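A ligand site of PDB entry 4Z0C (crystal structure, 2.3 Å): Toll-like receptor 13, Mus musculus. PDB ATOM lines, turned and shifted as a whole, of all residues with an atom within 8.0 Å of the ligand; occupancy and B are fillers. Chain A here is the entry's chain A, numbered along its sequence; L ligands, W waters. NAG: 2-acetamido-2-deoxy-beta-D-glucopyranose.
The backbone NH (N) of His 265 lies within hydrogen-bond range of an oxygen (O6) of the ligand (2.9 Å).
A ring nitrogen (ND1) of His 265 sits close to an oxygen (O6) of the ligand (3.4 Å).
O5 of the ligand lies close to ND2 of Asn 289.
The backbone NH of His 265 lies within hydrogen-bond range of the backbone carbonyl oxygen of Asn 289 (3.4 Å).
The side-chain carboxylate (OD2) of Asp 315 sits close to a ring nitrogen (NE2) of His 265, at 3.0 Å.
The side-chain amide nitrogen (ND2) of Asn 289 is in hydrogen-bond range of the backbone carbonyl oxygen (O) of Leu 261, at 2.4 Å.
The backbone carbonyl oxygen of Asn 289 sits at hydrogen-bond distance from the side-chain amide nitrogen of Asn 258 (3.3 Å).
The backbone NH (N) of Asn 289 lies within hydrogen-bond range of the backbone carbonyl oxygen (O) of Gln 312, 3.1 Å away.
OD1 of Asn 313 sits at hydrogen-bond distance from N of Asn 289 (3.0 Å).
O of Gly 264 sits at hydrogen-bond distance from ND2 of Asn 258, at 3.0 Å.
O of Leu 261 lies close to O7 of the ligand, 3.5 Å away.
Merely in contact with the ligand: Asp 315, Ser 314, Gly 264 and Arg 262.
Hydrophobic or aromatic side chains that line the ligand: Leu 261 and His 265.
Seven residues have an atom within 4 Å of the ligand: Leu 261, Arg 262, Gly 264, His 265, Asn 289, Ser 314 and Asp 315.
The nearest printed residue that does not touch the ligand is His 263 (5.4 Å).
Water W1 lies within hydrogen-bond range of the side-chain carboxylate (OD1) of Asp 315 (2.5 Å), the side-chain hydroxyl (OG) of Ser 314 (2.6 Å) and a nitrogen (N2) of the ligand (2.8 Å).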
ATOM      1  N   ASN A 258      34.455   9.678  19.962  1.00  0.00           N
ATOM      2  CA  ASN A 258      34.531   9.997  21.382  1.00  0.00           C
ATOM      3  C   ASN A 258      35.143   8.826  22.146  1.00  0.00           C
ATOM      4  O   ASN A 258      35.186   7.716  21.635  1.00  0.00           O
ATOM      5  CB  ASN A 258      33.136  10.257  21.943  1.00  0.00           C
ATOM      6  CG  ASN A 258      32.523  11.523  21.416  1.00  0.00           C
ATOM      7  OD1 ASN A 258      33.223  12.473  21.080  1.00  0.00           O
ATOM      8  ND2 ASN A 258      31.188  11.542  21.322  1.00  0.00           N
ATOM      9  N   GLU A 260      33.711   7.993  25.280  1.00  0.00           N
ATOM     10  CA  GLU A 260      32.423   7.498  25.765  1.00  0.00           C
ATOM     11  C   GLU A 260      31.244   8.276  25.178  1.00  0.00           C
ATOM     12  O   GLU A 260      31.401   9.401  24.696  1.00  0.00           O
ATOM     13  CB  GLU A 260      32.349   7.547  27.299  1.00  0.00           C
ATOM     14  CG  GLU A 260      33.264   6.588  28.014  1.00  0.00           C
ATOM     15  CD  GLU A 260      32.993   5.129  27.646  1.00  0.00           C
ATOM     16  OE1 GLU A 260      31.829   4.817  27.288  1.00  0.00           O
ATOM     17  OE2 GLU A 260      33.938   4.305  27.713  1.00  0.00           O
ATOM     18  N   LEU A 261      30.070   7.658  25.207  1.00  0.00           N
ATOM     19  CA  LEU A 261      28.857   8.243  24.675  1.00  0.00           C
ATOM     20  C   LEU A 261      28.527   9.559  25.391  1.00  0.00           C
ATOM     21  O   LEU A 261      28.021  10.502  24.769  1.00  0.00           O
ATOM     22  CB  LEU A 261      27.694   7.243  24.796  1.00  0.00           C
ATOM     23  CG  LEU A 261      27.883   5.877  24.110  1.00  0.00           C
ATOM     24  CD1 LEU A 261      26.701   4.908  24.365  1.00  0.00           C
ATOM     25  CD2 LEU A 261      28.099   6.042  22.627  1.00  0.00           C
ATOM     26  N   ARG A 262      28.802   9.599  26.699  1.00  0.00           N
ATOM     27  CA  ARG A 262      28.592  10.786  27.539  1.00  0.00           C
ATOM     28  C   ARG A 262      29.107  12.063  26.900  1.00  0.00           C
ATOM     29  O   ARG A 262      28.508  13.117  27.062  1.00  0.00           O
ATOM     30  CB  ARG A 262      29.312  10.637  28.882  1.00  0.00           C
ATOM     31  CG  ARG A 262      28.633   9.790  29.915  1.00  0.00           C
ATOM     32  CD  ARG A 262      29.462   9.769  31.195  1.00  0.00           C
ATOM     33  NE  ARG A 262      30.841   9.401  30.922  1.00  0.00           N
ATOM     34  CZ  ARG A 262      31.290   8.145  30.854  1.00  0.00           C
ATOM     35  NH1 ARG A 262      32.568   7.903  30.587  1.00  0.00           N
ATOM     36  NH2 ARG A 262      30.448   7.129  31.036  1.00  0.00           N
ATOM     37  N   HIS A 263      30.228  11.968  26.205  1.00  0.00           N
ATOM     38  CA  HIS A 263      30.899  13.156  25.697  1.00  0.00           C
ATOM     39  C   HIS A 263      30.002  13.969  24.750  1.00  0.00           C
ATOM     40  O   HIS A 263      30.091  15.187  24.665  1.00  0.00           O
ATOM     41  CB  HIS A 263      32.254  12.828  25.072  1.00  0.00           C
ATOM     42  CG  HIS A 263      33.221  13.984  25.121  1.00  0.00           C
ATOM     43  ND1 HIS A 263      33.307  14.923  24.112  1.00  0.00           N
ATOM     44  CD2 HIS A 263      34.102  14.357  26.076  1.00  0.00           C
ATOM     45  CE1 HIS A 263      34.223  15.819  24.437  1.00  0.00           C
ATOM     46  NE2 HIS A 263      34.711  15.507  25.630  1.00  0.00           N
ATOM     47  N   GLY A 264      29.119  13.277  24.036  1.00  0.00           N
ATOM     48  CA  GLY A 264      28.106  13.968  23.257  1.00  0.00           C
ATOM     49  C   GLY A 264      28.521  14.347  21.853  1.00  0.00           C
ATOM     50  O   GLY A 264      29.672  14.154  21.465  1.00  0.00           O
ATOM     51  N   HIS A 265      27.586  14.898  21.106  1.00  0.00           N
ATOM     52  CA  HIS A 265      27.799  15.205  19.698  1.00  0.00           C
ATOM     53  C   HIS A 265      28.919  16.228  19.512  1.00  0.00           C
ATOM     54  O   HIS A 265      29.150  17.074  20.378  1.00  0.00           O
ATOM     55  CB  HIS A 265      26.522  15.769  19.070  1.00  0.00           C
ATOM     56  CG  HIS A 265      25.310  14.901  19.246  1.00  0.00           C
ATOM     57  ND1 HIS A 265      25.386  13.613  19.727  1.00  0.00           N
ATOM     58  CD2 HIS A 265      24.005  15.152  19.021  1.00  0.00           C
ATOM     59  CE1 HIS A 265      24.165  13.102  19.783  1.00  0.00           C
ATOM     60  NE2 HIS A 265      23.309  14.009  19.351  1.00  0.00           N
ATOM     61  N   LEU A 266      29.615  16.129  18.388  1.00  0.00           N
ATOM     62  CA  LEU A 266      30.605  17.128  17.997  1.00  0.00           C
ATOM     63  C   LEU A 266      29.892  18.255  17.253  1.00  0.00           C
ATOM     64  O   LEU A 266      28.852  18.031  16.637  1.00  0.00           O
ATOM     65  CB  LEU A 266      31.682  16.509  17.104  1.00  0.00           C
ATOM     66  CG  LEU A 266      32.685  15.495  17.682  1.00  0.00           C
ATOM     67  CD1 LEU A 266      33.715  15.007  16.626  1.00  0.00           C
ATOM     68  CD2 LEU A 266      33.387  16.080  18.908  1.00  0.00           C
ATOM     69  N   LYS A 288      30.689   6.557  18.539  1.00  0.00           N
ATOM     70  CA  LYS A 288      30.352   6.742  19.950  1.00  0.00           C
ATOM     71  C   LYS A 288      29.633   8.057  20.260  1.00  0.00           C
ATOM     72  O   LYS A 288      30.082   8.873  21.058  1.00  0.00           O
ATOM     73  CB  LYS A 288      31.561   6.511  20.890  1.00  0.00           C
ATOM     74  CG  LYS A 288      31.984   5.045  20.961  1.00  0.00           C
ATOM     75  CD  LYS A 288      33.065   4.797  22.026  1.00  0.00           C
ATOM     76  CE  LYS A 288      33.802   3.474  21.797  1.00  0.00           C
ATOM     77  NZ  LYS A 288      34.959   3.264  22.725  1.00  0.00           N
ATOM     78  N   ASN A 289      28.484   8.228  19.615  1.00  0.00           N
ATOM     79  CA  ASN A 289      27.561   9.296  19.975  1.00  0.00           C
ATOM     80  C   ASN A 289      28.148  10.655  19.630  1.00  0.00           C
ATOM     81  O   ASN A 289      28.062  11.628  20.366  1.00  0.00           O
ATOM     82  CB  ASN A 289      27.229   9.209  21.464  1.00  0.00           C
ATOM     83  CG  ASN A 289      26.166  10.152  21.884  1.00  0.00           C
ATOM     84  OD1 ASN A 289      25.212  10.431  21.148  1.00  0.00           O
ATOM     85  ND2 ASN A 289      26.333  10.705  23.075  1.00  0.00           N
ATOM     86  N   VAL A 290      28.737  10.673  18.442  1.00  0.00           N
ATOM     87  CA  VAL A 290      29.438  11.847  17.982  1.00  0.00           C
ATOM     88  C   VAL A 290      28.474  12.682  17.098  1.00  0.00           C
ATOM     89  O   VAL A 290      28.657  13.874  16.933  1.00  0.00           O
ATOM     90  CB  VAL A 290      30.740  11.376  17.264  1.00  0.00           C
ATOM     91  CG1 VAL A 290      30.779  11.787  15.820  1.00  0.00           C
ATOM     92  CG2 VAL A 290      31.954  11.874  18.009  1.00  0.00           C
ATOM     93  N   THR A 291      27.411  12.053  16.615  1.00  0.00           N
ATOM     94  CA  THR A 291      26.463  12.724  15.720  1.00  0.00           C
ATOM     95  C   THR A 291      25.056  12.108  15.762  1.00  0.00           C
ATOM     96  O   THR A 291      24.851  11.065  16.368  1.00  0.00           O
ATOM     97  CB  THR A 291      26.956  12.687  14.262  1.00  0.00           C
ATOM     98  OG1 THR A 291      26.143  13.545  13.444  1.00  0.00           O
ATOM     99  CG2 THR A 291      26.866  11.275  13.721  1.00  0.00           C
ATOM    100  N   ASN A 292      24.099  12.781  15.148  1.00  0.00           N
ATOM    101  CA  ASN A 292      22.795  12.193  14.861  1.00  0.00           C
ATOM    102  C   ASN A 292      22.503  12.217  13.362  1.00  0.00           C
ATOM    103  O   ASN A 292      23.391  12.525  12.582  1.00  0.00           O
ATOM    104  CB  ASN A 292      21.657  12.817  15.706  1.00  0.00           C
ATOM    105  CG  ASN A 292      21.489  14.325  15.517  1.00  0.00           C
ATOM    106  OD1 ASN A 292      21.910  14.926  14.517  1.00  0.00           O
ATOM    107  ND2 ASN A 292      20.822  14.946  16.490  1.00  0.00           N
ATOM    108  N   GLN A 312      28.286   2.761  16.878  1.00  0.00           N
ATOM    109  CA  GLN A 312      28.043   3.189  18.255  1.00  0.00           C
ATOM    110  C   GLN A 312      27.466   4.611  18.382  1.00  0.00           C
ATOM    111  O   GLN A 312      27.665   5.270  19.405  1.00  0.00           O
ATOM    112  CB  GLN A 312      29.304   3.055  19.117  1.00  0.00           C
ATOM    113  CG  GLN A 312      29.780   1.617  19.327  1.00  0.00           C
ATOM    114  CD  GLN A 312      31.000   1.539  20.212  1.00  0.00           C
ATOM    115  OE1 GLN A 312      32.129   1.567  19.736  1.00  0.00           O
ATOM    116  NE2 GLN A 312      30.777   1.521  21.521  1.00  0.00           N
ATOM    117  N   ASN A 313      26.771   5.079  17.361  1.00  0.00           N
ATOM    118  CA  ASN A 313      26.005   6.328  17.483  1.00  0.00           C
ATOM    119  C   ASN A 313      24.600   6.077  18.003  1.00  0.00           C
ATOM    120  O   ASN A 313      23.659   5.854  17.229  1.00  0.00           O
ATOM    121  CB  ASN A 313      26.023   7.115  16.179  1.00  0.00           C
ATOM    122  CG  ASN A 313      27.351   7.832  15.976  1.00  0.00           C
ATOM    123  OD1 ASN A 313      27.707   8.719  16.745  1.00  0.00           O
ATOM    124  ND2 ASN A 313      28.104   7.421  14.944  1.00  0.00           N
ATOM    125  N   SER A 314      24.480   6.128  19.330  1.00  0.00           N
ATOM    126  CA  SER A 314      23.278   5.721  20.031  1.00  0.00           C
ATOM    127  C   SER A 314      22.010   6.519  19.680  1.00  0.00           C
ATOM    128  O   SER A 314      20.896   6.060  19.922  1.00  0.00           O
ATOM    129  CB  SER A 314      23.546   5.751  21.539  1.00  0.00           C
ATOM    130  OG  SER A 314      24.268   6.916  21.914  1.00  0.00           O
ATOM    131  N   ASP A 315      22.184   7.711  19.113  1.00  0.00           N
ATOM    132  CA  ASP A 315      21.029   8.516  18.714  1.00  0.00           C
ATOM    133  C   ASP A 315      20.488   8.205  17.329  1.00  0.00           C
ATOM    134  O   ASP A 315      19.539   8.846  16.852  1.00  0.00           O
ATOM    135  CB  ASP A 315      21.337  10.015  18.819  1.00  0.00           C
ATOM    136  CG  ASP A 315      21.288  10.524  20.253  1.00  0.00           C
ATOM    137  OD1 ASP A 315      20.748   9.809  21.131  1.00  0.00           O
ATOM    138  OD2 ASP A 315      21.794  11.641  20.509  1.00  0.00           O
ATOM    139  N   GLN A 339      21.392   2.217  17.639  1.00  0.00           N
ATOM    140  CA  GLN A 339      20.105   1.773  18.199  1.00  0.00           C
ATOM    141  C   GLN A 339      19.050   1.680  17.102  1.00  0.00           C
ATOM    142  O   GLN A 339      17.889   1.913  17.342  1.00  0.00           O
ATOM    143  CB  GLN A 339      19.643   2.735  19.284  1.00  0.00           C
ATOM    144  CG  GLN A 339      20.595   2.856  20.464  1.00  0.00           C
ATOM    145  CD  GLN A 339      20.604   1.606  21.317  1.00  0.00           C
ATOM    146  OE1 GLN A 339      19.553   1.055  21.640  1.00  0.00           O
ATOM    147  NE2 GLN A 339      21.786   1.127  21.675  1.00  0.00           N
HETATM  148  C1  NAG L   1      23.676  11.901  23.265  1.00  0.00           C
HETATM  149  C2  NAG L   1      23.866  11.382  24.670  1.00  0.00           C
HETATM  150  C3  NAG L   1      22.942  12.239  25.515  1.00  0.00           C
HETATM  151  C4  NAG L   1      23.343  13.714  25.353  1.00  0.00           C
HETATM  152  C5  NAG L   1      23.793  14.098  23.920  1.00  0.00           C
HETATM  153  C6  NAG L   1      24.726  15.304  23.888  1.00  0.00           C
HETATM  154  C7  NAG L   1      24.293   9.111  25.462  1.00  0.00           C
HETATM  155  C8  NAG L   1      24.032   7.653  25.236  1.00  0.00           C
HETATM  156  N2  NAG L   1      23.596   9.954  24.712  1.00  0.00           N
HETATM  157  O3  NAG L   1      23.011  11.797  26.855  1.00  0.00           O
HETATM  158  O4  NAG L   1      22.251  14.541  25.734  1.00  0.00           O
HETATM  159  O5  NAG L   1      24.470  13.063  23.230  1.00  0.00           O
HETATM  160  O6  NAG L   1      25.132  15.521  22.550  1.00  0.00           O
HETATM  161  O7  NAG L   1      25.090   9.465  26.325  1.00  0.00           O
HETATM  162  O   HOH W   1      22.374   8.618  22.623  1.00  0.00           O
HETATM  163  O   HOH W   2      21.343  17.039  25.097  1.00  0.00           O
